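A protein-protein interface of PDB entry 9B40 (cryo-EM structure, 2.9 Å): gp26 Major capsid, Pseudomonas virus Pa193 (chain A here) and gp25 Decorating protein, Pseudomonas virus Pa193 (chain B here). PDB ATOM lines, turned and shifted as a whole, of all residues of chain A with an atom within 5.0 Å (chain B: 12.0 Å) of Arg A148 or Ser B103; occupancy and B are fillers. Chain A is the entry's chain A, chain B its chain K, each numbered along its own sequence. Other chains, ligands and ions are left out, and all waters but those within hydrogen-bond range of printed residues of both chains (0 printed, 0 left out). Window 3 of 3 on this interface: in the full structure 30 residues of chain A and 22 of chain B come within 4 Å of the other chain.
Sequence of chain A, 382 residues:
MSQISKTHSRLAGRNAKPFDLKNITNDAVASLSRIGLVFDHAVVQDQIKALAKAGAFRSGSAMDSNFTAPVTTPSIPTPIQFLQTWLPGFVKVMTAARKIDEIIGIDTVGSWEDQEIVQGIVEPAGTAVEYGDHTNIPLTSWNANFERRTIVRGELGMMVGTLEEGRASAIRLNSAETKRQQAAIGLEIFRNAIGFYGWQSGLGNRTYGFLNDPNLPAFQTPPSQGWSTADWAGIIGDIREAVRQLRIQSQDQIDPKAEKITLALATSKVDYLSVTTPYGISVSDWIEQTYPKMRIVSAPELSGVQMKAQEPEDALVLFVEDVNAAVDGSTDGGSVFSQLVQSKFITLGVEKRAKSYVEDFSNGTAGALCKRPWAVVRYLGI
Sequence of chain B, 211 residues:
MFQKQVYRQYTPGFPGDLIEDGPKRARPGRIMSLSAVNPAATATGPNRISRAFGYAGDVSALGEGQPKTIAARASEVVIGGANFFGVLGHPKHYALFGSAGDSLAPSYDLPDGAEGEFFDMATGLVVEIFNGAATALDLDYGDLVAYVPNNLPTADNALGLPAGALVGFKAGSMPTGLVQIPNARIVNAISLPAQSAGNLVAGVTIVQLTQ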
ATOM      1  N   GLU A 116      20.083  -3.826 -14.593  1.00  0.00           N
ATOM      2  CA  GLU A 116      19.527  -3.233 -15.801  1.00  0.00           C
ATOM      3  C   GLU A 116      20.629  -2.632 -16.661  1.00  0.00           C
ATOM      4  O   GLU A 116      21.712  -2.290 -16.182  1.00  0.00           O
ATOM      5  CB  GLU A 116      18.488  -2.152 -15.473  1.00  0.00           C
ATOM      6  CG  GLU A 116      17.101  -2.685 -15.169  1.00  0.00           C
ATOM      7  CD  GLU A 116      16.109  -1.581 -14.866  1.00  0.00           C
ATOM      8  OE1 GLU A 116      16.441  -0.404 -15.112  1.00  0.00           O
ATOM      9  OE2 GLU A 116      14.999  -1.889 -14.381  1.00  0.00           O
ATOM     10  N   ILE A 117      20.325  -2.516 -17.950  1.00  0.00           N
ATOM     11  CA  ILE A 117      21.149  -1.823 -18.933  1.00  0.00           C
ATOM     12  C   ILE A 117      20.295  -0.763 -19.611  1.00  0.00           C
ATOM     13  O   ILE A 117      19.162  -1.039 -20.020  1.00  0.00           O
ATOM     14  CB  ILE A 117      21.747  -2.797 -19.967  1.00  0.00           C
ATOM     15  CG1 ILE A 117      22.916  -3.570 -19.354  1.00  0.00           C
ATOM     16  CG2 ILE A 117      22.124  -2.083 -21.253  1.00  0.00           C
ATOM     17  CD1 ILE A 117      23.841  -4.173 -20.375  1.00  0.00           C
ATOM     18  N   VAL A 118      20.840   0.448 -19.725  1.00  0.00           N
ATOM     19  CA  VAL A 118      20.128   1.597 -20.267  1.00  0.00           C
ATOM     20  C   VAL A 118      20.806   2.035 -21.558  1.00  0.00           C
ATOM     21  O   VAL A 118      22.036   2.143 -21.615  1.00  0.00           O
ATOM     22  CB  VAL A 118      20.084   2.757 -19.258  1.00  0.00           C
ATOM     23  CG1 VAL A 118      19.181   3.860 -19.765  1.00  0.00           C
ATOM     24  CG2 VAL A 118      19.610   2.254 -17.912  1.00  0.00           C
ATOM     25  N   PHE A 146      15.445   7.375 -22.908  1.00  0.00           N
ATOM     26  CA  PHE A 146      16.238   6.255 -22.426  1.00  0.00           C
ATOM     27  C   PHE A 146      15.382   5.000 -22.365  1.00  0.00           C
ATOM     28  O   PHE A 146      14.193   5.055 -22.045  1.00  0.00           O
ATOM     29  CB  PHE A 146      16.839   6.559 -21.049  1.00  0.00           C
ATOM     30  CG  PHE A 146      17.537   7.885 -20.977  1.00  0.00           C
ATOM     31  CD1 PHE A 146      18.792   8.054 -21.532  1.00  0.00           C
ATOM     32  CD2 PHE A 146      16.927   8.970 -20.373  1.00  0.00           C
ATOM     33  CE1 PHE A 146      19.434   9.274 -21.472  1.00  0.00           C
ATOM     34  CE2 PHE A 146      17.562  10.192 -20.314  1.00  0.00           C
ATOM     35  CZ  PHE A 146      18.817  10.344 -20.863  1.00  0.00           C
ATOM     36  N   GLU A 147      16.010   3.864 -22.657  1.00  0.00           N
ATOM     37  CA  GLU A 147      15.354   2.565 -22.637  1.00  0.00           C
ATOM     38  C   GLU A 147      16.112   1.637 -21.704  1.00  0.00           C
ATOM     39  O   GLU A 147      17.332   1.499 -21.819  1.00  0.00           O
ATOM     40  CB  GLU A 147      15.279   1.956 -24.040  1.00  0.00           C
ATOM     41  CG  GLU A 147      14.576   0.601 -24.127  1.00  0.00           C
ATOM     42  CD  GLU A 147      13.081   0.657 -23.852  1.00  0.00           C
ATOM     43  OE1 GLU A 147      12.678   0.886 -22.693  1.00  0.00           O
ATOM     44  OE2 GLU A 147      12.299   0.461 -24.807  1.00  0.00           O
ATOM     45  N   ARG A 148      15.387   0.993 -20.796  1.00  0.00           N
ATOM     46  CA  ARG A 148      15.972   0.111 -19.798  1.00  0.00           C
ATOM     47  C   ARG A 148      15.566  -1.330 -20.078  1.00  0.00           C
ATOM     48  O   ARG A 148      14.437  -1.600 -20.501  1.00  0.00           O
ATOM     49  CB  ARG A 148      15.553   0.538 -18.384  1.00  0.00           C
ATOM     50  CG  ARG A 148      14.085   0.310 -18.059  1.00  0.00           C
ATOM     51  CD  ARG A 148      13.614   1.123 -16.864  1.00  0.00           C
ATOM     52  NE  ARG A 148      14.620   1.256 -15.817  1.00  0.00           N
ATOM     53  CZ  ARG A 148      14.406   1.868 -14.661  1.00  0.00           C
ATOM     54  NH1 ARG A 148      13.240   2.424 -14.379  1.00  0.00           N
ATOM     55  NH2 ARG A 148      15.388   1.924 -13.766  1.00  0.00           N
ATOM     56  N   ARG A 149      16.512  -2.248 -19.893  1.00  0.00           N
ATOM     57  CA  ARG A 149      16.277  -3.678 -20.056  1.00  0.00           C
ATOM     58  C   ARG A 149      16.940  -4.415 -18.907  1.00  0.00           C
ATOM     59  O   ARG A 149      18.128  -4.210 -18.646  1.00  0.00           O
ATOM     60  CB  ARG A 149      16.826  -4.186 -21.390  1.00  0.00           C
ATOM     61  CG  ARG A 149      16.183  -3.539 -22.585  1.00  0.00           C
ATOM     62  CD  ARG A 149      14.801  -4.101 -22.804  1.00  0.00           C
ATOM     63  NE  ARG A 149      14.589  -4.398 -24.211  1.00  0.00           N
ATOM     64  CZ  ARG A 149      13.977  -3.581 -25.053  1.00  0.00           C
ATOM     65  NH1 ARG A 149      13.420  -2.456 -24.642  1.00  0.00           N
ATOM     66  NH2 ARG A 149      13.921  -3.901 -26.340  1.00  0.00           N
ATOM     67  N   THR A 150      16.189  -5.280 -18.233  1.00  0.00           N
ATOM     68  CA  THR A 150      16.745  -5.952 -17.072  1.00  0.00           C
ATOM     69  C   THR A 150      17.727  -7.044 -17.502  1.00  0.00           C
ATOM     70  O   THR A 150      17.927  -7.310 -18.688  1.00  0.00           O
ATOM     71  CB  THR A 150      15.639  -6.528 -16.188  1.00  0.00           C
ATOM     72  OG1 THR A 150      15.097  -7.705 -16.791  1.00  0.00           O
ATOM     73  CG2 THR A 150      14.532  -5.506 -15.991  1.00  0.00           C
ATOM     74  N   ARG A 206      10.754  -7.521 -18.565  1.00  0.00           N
ATOM     75  CA  ARG A 206      11.454  -6.504 -19.358  1.00  0.00           C
ATOM     76  C   ARG A 206      12.777  -7.035 -19.909  1.00  0.00           C
ATOM     77  O   ARG A 206      13.789  -6.334 -19.931  1.00  0.00           O
ATOM     78  CB  ARG A 206      11.669  -5.219 -18.555  1.00  0.00           C
ATOM     79  CG  ARG A 206      10.413  -4.387 -18.379  1.00  0.00           C
ATOM     80  CD  ARG A 206      10.084  -3.592 -19.626  1.00  0.00           C
ATOM     81  NE  ARG A 206      11.030  -2.500 -19.824  1.00  0.00           N
ATOM     82  CZ  ARG A 206      11.055  -1.712 -20.889  1.00  0.00           C
ATOM     83  NH1 ARG A 206      10.202  -1.873 -21.888  1.00  0.00           N
ATOM     84  NH2 ARG A 206      11.956  -0.737 -20.952  1.00  0.00           N
ATOM     85  N   MET B   1      10.641   3.522 -28.502  1.00  0.00           N
ATOM     86  CA  MET B   1      11.608   4.341 -27.723  1.00  0.00           C
ATOM     87  C   MET B   1      12.553   5.062 -28.689  1.00  0.00           C
ATOM     88  O   MET B   1      12.656   6.302 -28.602  1.00  0.00           O
ATOM     89  CB  MET B   1      12.433   3.462 -26.779  1.00  0.00           C
ATOM     90  CG  MET B   1      13.561   4.209 -26.096  1.00  0.00           C
ATOM     91  SD  MET B   1      12.946   5.521 -25.014  1.00  0.00           S
ATOM     92  CE  MET B   1      11.690   4.627 -24.098  1.00  0.00           C
ATOM     93  N   PHE B   2      13.211   4.307 -29.572  1.00  0.00           N
ATOM     94  CA  PHE B   2      14.157   4.907 -30.548  1.00  0.00           C
ATOM     95  C   PHE B   2      13.401   5.272 -31.829  1.00  0.00           C
ATOM     96  O   PHE B   2      12.175   5.057 -31.885  1.00  0.00           O
ATOM     97  CB  PHE B   2      15.307   3.939 -30.834  1.00  0.00           C
ATOM     98  CG  PHE B   2      15.815   3.191 -29.626  1.00  0.00           C
ATOM     99  CD1 PHE B   2      15.259   1.978 -29.254  1.00  0.00           C
ATOM    100  CD2 PHE B   2      16.853   3.700 -28.863  1.00  0.00           C
ATOM    101  CE1 PHE B   2      15.726   1.295 -28.142  1.00  0.00           C
ATOM    102  CE2 PHE B   2      17.319   3.016 -27.752  1.00  0.00           C
ATOM    103  CZ  PHE B   2      16.757   1.813 -27.395  1.00  0.00           C
ATOM    104  N   TYR B  94      16.499  21.583 -16.096  1.00  0.00           N
ATOM    105  CA  TYR B  94      15.876  20.777 -15.057  1.00  0.00           C
ATOM    106  C   TYR B  94      16.363  19.334 -15.099  1.00  0.00           C
ATOM    107  O   TYR B  94      17.092  18.914 -16.001  1.00  0.00           O
ATOM    108  CB  TYR B  94      14.354  20.841 -15.198  1.00  0.00           C
ATOM    109  CG  TYR B  94      13.880  22.200 -15.648  1.00  0.00           C
ATOM    110  CD1 TYR B  94      14.085  23.315 -14.855  1.00  0.00           C
ATOM    111  CD2 TYR B  94      13.277  22.378 -16.880  1.00  0.00           C
ATOM    112  CE1 TYR B  94      13.679  24.562 -15.259  1.00  0.00           C
ATOM    113  CE2 TYR B  94      12.868  23.627 -17.293  1.00  0.00           C
ATOM    114  CZ  TYR B  94      13.070  24.714 -16.478  1.00  0.00           C
ATOM    115  OH  TYR B  94      12.665  25.961 -16.884  1.00  0.00           O
ATOM    116  N   ALA B  95      15.953  18.577 -14.086  1.00  0.00           N
ATOM    117  CA  ALA B  95      16.322  17.177 -13.930  1.00  0.00           C
ATOM    118  C   ALA B  95      15.101  16.299 -14.158  1.00  0.00           C
ATOM    119  O   ALA B  95      14.021  16.581 -13.630  1.00  0.00           O
ATOM    120  CB  ALA B  95      16.901  16.919 -12.539  1.00  0.00           C
ATOM    121  N   LEU B  96      15.276  15.240 -14.943  1.00  0.00           N
ATOM    122  CA  LEU B  96      14.194  14.297 -15.178  1.00  0.00           C
ATOM    123  C   LEU B  96      13.989  13.420 -13.949  1.00  0.00           C
ATOM    124  O   LEU B  96      14.940  12.835 -13.426  1.00  0.00           O
ATOM    125  CB  LEU B  96      14.503  13.433 -16.398  1.00  0.00           C
ATOM    126  CG  LEU B  96      13.576  12.255 -16.686  1.00  0.00           C
ATOM    127  CD1 LEU B  96      12.159  12.737 -16.913  1.00  0.00           C
ATOM    128  CD2 LEU B  96      14.078  11.476 -17.884  1.00  0.00           C
ATOM    129  N   PHE B  97      12.742  13.327 -13.494  1.00  0.00           N
ATOM    130  CA  PHE B  97      12.391  12.510 -12.341  1.00  0.00           C
ATOM    131  C   PHE B  97      11.625  11.253 -12.720  1.00  0.00           C
ATOM    132  O   PHE B  97      11.281  10.464 -11.835  1.00  0.00           O
ATOM    133  CB  PHE B  97      11.567  13.331 -11.343  1.00  0.00           C
ATOM    134  CG  PHE B  97      12.391  14.227 -10.469  1.00  0.00           C
ATOM    135  CD1 PHE B  97      12.968  13.745  -9.308  1.00  0.00           C
ATOM    136  CD2 PHE B  97      12.587  15.555 -10.807  1.00  0.00           C
ATOM    137  CE1 PHE B  97      13.727  14.570  -8.500  1.00  0.00           C
ATOM    138  CE2 PHE B  97      13.345  16.384 -10.006  1.00  0.00           C
ATOM    139  CZ  PHE B  97      13.915  15.891  -8.850  1.00  0.00           C
ATOM    140  N   GLY B  98      11.353  11.043 -14.000  1.00  0.00           N
ATOM    141  CA  GLY B  98      10.556   9.918 -14.422  1.00  0.00           C
ATOM    142  C   GLY B  98       9.079  10.147 -14.170  1.00  0.00           C
ATOM    143  O   GLY B  98       8.632  11.241 -13.815  1.00  0.00           O
ATOM    144  N   SER B  99       8.307   9.078 -14.360  1.00  0.00           N
ATOM    145  CA  SER B  99       6.859   9.142 -14.179  1.00  0.00           C
ATOM    146  C   SER B  99       6.379   7.805 -13.636  1.00  0.00           C
ATOM    147  O   SER B  99       6.426   6.797 -14.349  1.00  0.00           O
ATOM    148  CB  SER B  99       6.149   9.482 -15.487  1.00  0.00           C
ATOM    149  OG  SER B  99       6.895  10.399 -16.268  1.00  0.00           O
ATOM    150  N   ALA B 100       5.926   7.807 -12.378  1.00  0.00           N
ATOM    151  CA  ALA B 100       5.253   6.670 -11.743  1.00  0.00           C
ATOM    152  C   ALA B 100       6.137   5.420 -11.725  1.00  0.00           C
ATOM    153  O   ALA B 100       5.829   4.395 -12.337  1.00  0.00           O
ATOM    154  CB  ALA B 100       3.906   6.387 -12.419  1.00  0.00           C
ATOM    155  N   GLY B 101       7.241   5.524 -11.011  1.00  0.00           N
ATOM    156  CA  GLY B 101       8.138   4.386 -10.826  1.00  0.00           C
ATOM    157  C   GLY B 101       9.240   4.248 -11.850  1.00  0.00           C
ATOM    158  O   GLY B 101      10.394   4.015 -11.494  1.00  0.00           O
ATOM    159  N   ASP B 102       8.899   4.383 -13.128  1.00  0.00           N
ATOM    160  CA  ASP B 102       9.894   4.335 -14.196  1.00  0.00           C
ATOM    161  C   ASP B 102      10.679   5.638 -14.167  1.00  0.00           C
ATOM    162  O   ASP B 102      10.223   6.665 -14.672  1.00  0.00           O
ATOM    163  CB  ASP B 102       9.223   4.113 -15.545  1.00  0.00           C
ATOM    164  CG  ASP B 102      10.168   3.534 -16.580  1.00  0.00           C
ATOM    165  OD1 ASP B 102      11.399   3.660 -16.407  1.00  0.00           O
ATOM    166  OD2 ASP B 102       9.681   2.947 -17.569  1.00  0.00           O
ATOM    167  N   SER B 103      11.868   5.599 -13.562  1.00  0.00           N
ATOM    168  CA  SER B 103      12.663   6.806 -13.371  1.00  0.00           C
ATOM    169  C   SER B 103      13.191   7.378 -14.679  1.00  0.00           C
ATOM    170  O   SER B 103      13.585   8.549 -14.714  1.00  0.00           O
ATOM    171  CB  SER B 103      13.826   6.518 -12.423  1.00  0.00           C
ATOM    172  OG  SER B 103      14.269   5.179 -12.553  1.00  0.00           O
ATOM    173  N   LEU B 104      13.219   6.587 -15.748  1.00  0.00           N
ATOM    174  CA  LEU B 104      13.690   7.044 -17.046  1.00  0.00           C
ATOM    175  C   LEU B 104      12.550   7.335 -18.011  1.00  0.00           C
ATOM    176  O   LEU B 104      12.801   7.556 -19.199  1.00  0.00           O
ATOM    177  CB  LEU B 104      14.641   6.011 -17.647  1.00  0.00           C
ATOM    178  CG  LEU B 104      15.775   5.586 -16.716  1.00  0.00           C
ATOM    179  CD1 LEU B 104      16.529   4.408 -17.294  1.00  0.00           C
ATOM    180  CD2 LEU B 104      16.714   6.751 -16.460  1.00  0.00           C
ATOM    181  N   ALA B 105      11.309   7.333 -17.531  1.00  0.00           N
ATOM    182  CA  ALA B 105      10.172   7.625 -18.387  1.00  0.00           C
ATOM    183  C   ALA B 105      10.197   9.088 -18.822  1.00  0.00           C
ATOM    184  O   ALA B 105      10.602   9.965 -18.055  1.00  0.00           O
ATOM    185  CB  ALA B 105       8.865   7.321 -17.662  1.00  0.00           C
ATOM    186  N   PRO B 106       9.790   9.373 -20.060  1.00  0.00           N
ATOM    187  CA  PRO B 106       9.777  10.763 -20.532  1.00  0.00           C
ATOM    188  C   PRO B 106       8.804  11.619 -19.736  1.00  0.00           C
ATOM    189  O   PRO B 106       7.727  11.168 -19.341  1.00  0.00           O
ATOM    190  CB  PRO B 106       9.341  10.635 -21.995  1.00  0.00           C
ATOM    191  CG  PRO B 106       9.649   9.229 -22.370  1.00  0.00           C
ATOM    192  CD  PRO B 106       9.440   8.425 -21.129  1.00  0.00           C
ATOM    193  N   SER B 107       9.192  12.873 -19.514  1.00  0.00           N
ATOM    194  CA  SER B 107       8.376  13.792 -18.734  1.00  0.00           C
ATOM    195  C   SER B 107       8.753  15.219 -19.091  1.00  0.00           C
ATOM    196  O   SER B 107       9.928  15.586 -19.026  1.00  0.00           O
ATOM    197  CB  SER B 107       8.559  13.556 -17.231  1.00  0.00           C
ATOM    198  OG  SER B 107       7.638  14.326 -16.480  1.00  0.00           O
ATOM    199  N   TYR B 108       7.753  16.016 -19.458  1.00  0.00           N
ATOM    200  CA  TYR B 108       7.920  17.442 -19.696  1.00  0.00           C
ATOM    201  C   TYR B 108       7.265  18.272 -18.601  1.00  0.00           C
ATOM    202  O   TYR B 108       7.040  19.471 -18.781  1.00  0.00           O
ATOM    203  CB  TYR B 108       7.351  17.817 -21.064  1.00  0.00           C
ATOM    204  CG  TYR B 108       8.326  18.529 -21.966  1.00  0.00           C
ATOM    205  CD1 TYR B 108       9.685  18.267 -21.895  1.00  0.00           C
ATOM    206  CD2 TYR B 108       7.884  19.444 -22.909  1.00  0.00           C
ATOM    207  CE1 TYR B 108      10.580  18.908 -22.724  1.00  0.00           C
ATOM    208  CE2 TYR B 108       8.772  20.091 -23.743  1.00  0.00           C
ATOM    209  CZ  TYR B 108      10.118  19.819 -23.646  1.00  0.00           C
ATOM    210  OH  TYR B 108      11.008  20.458 -24.474  1.00  0.00           O
ATOM    211  N   ASP B 109       6.958  17.652 -17.467  1.00  0.00           N
ATOM    212  CA  ASP B 109       6.240  18.294 -16.378  1.00  0.00           C
ATOM    213  C   ASP B 109       7.200  18.604 -15.241  1.00  0.00           C
ATOM    214  O   ASP B 109       7.921  17.718 -14.770  1.00  0.00           O
ATOM    215  CB  ASP B 109       5.103  17.403 -15.881  1.00  0.00           C
ATOM    216  CG  ASP B 109       4.121  17.055 -16.975  1.00  0.00           C
ATOM    217  OD1 ASP B 109       3.789  17.951 -17.775  1.00  0.00           O
ATOM    218  OD2 ASP B 109       3.677  15.889 -17.037  1.00  0.00           O
ATOM    219  N   PRO B 111       7.927  19.342 -11.402  1.00  0.00           N
ATOM    220  CA  PRO B 111       7.247  19.076 -10.131  1.00  0.00           C
ATOM    221  C   PRO B 111       6.928  20.361  -9.387  1.00  0.00           C
ATOM    222  O   PRO B 111       7.549  21.404  -9.599  1.00  0.00           O
ATOM    223  CB  PRO B 111       8.258  18.220  -9.359  1.00  0.00           C
ATOM    224  CG  PRO B 111       9.574  18.574  -9.948  1.00  0.00           C
ATOM    225  CD  PRO B 111       9.317  18.859 -11.399  1.00  0.00           C
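Of chain B, only Asp B102, Ser B103 and Leu B104 come within 4 Å of Arg A148. Ser B103 touches one residue of chain A. No residue of chain B comes within 4 Å of Glu A116. Val A118 touches just one residue of chain B: Leu B104 (3.7 Å). No residue of chain B comes within 4 Å of Thr A150. No residue of chain B comes within 4 Å of Arg A206. Printed residues of chain A within 4 Å of Phe B2: Glu A147 (3.7 Å). Printed residues of chain A within 4 Å of Asp B102: Arg A148 (3.0 Å). Of the printed residues of chain A, Leu B104 touches Val A118 and Arg A148. Of the printed residues of chain B, Phe A146 touches Met B1. Printed residues of chain A within 4 Å of Met B1: Phe A146 and Glu A147. The nearest printed residue of chain A that does not touch Ser B103 is Glu A116 (6.5 Å).
Val A118 touches Leu B104 (CG1 to CD1, 3.7 Å). Glu A147 touches Met B1 (CB to CG, 3.5 Å). CZ of Phe B2 touches CB of Glu A147, at 3.7 Å. NE of Arg A148 touches CD1 of Leu B104, 3.97 Å away.
The side-chain carboxylate (OE1) of Glu A116 is in salt-bridge range of the guanidinium group (NE) of Arg A148 (2.6 Å). NH2 of Arg A206 lies within salt-bridge range of OE1 of Glu A147 (2.5 Å). O of Ser B103 sits close to N of Gly B98 (3.4 Å). The guanidinium group of Arg A149 is in salt-bridge range of the side-chain carboxylate of Glu A147 (3.1 Å). The guanidinium group of Arg A206 is in hydrogen-bond range of the backbone carbonyl oxygen of Arg A148.
N of Phe A146 sits close to SD of Met B1 (3.8 Å). The guanidinium group (NH1) of Arg A148 lies within salt-bridge range of the side-chain carboxylate (OD1) of Asp B102, at 3.0 Å. The side-chain hydroxyl (OG) of Ser B103 is in hydrogen-bond range of the guanidinium group (NH1) of Arg A148.
Of the 19 printed residues of chain B, 5 touch a printed residue of chain A. Hydrophobic or aromatic side chains of chain B that line the printed part of chain A: Met B1, Phe B2 and Leu B104. Of the 9 printed residues of chain A, 4 touch a printed residue of chain B.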
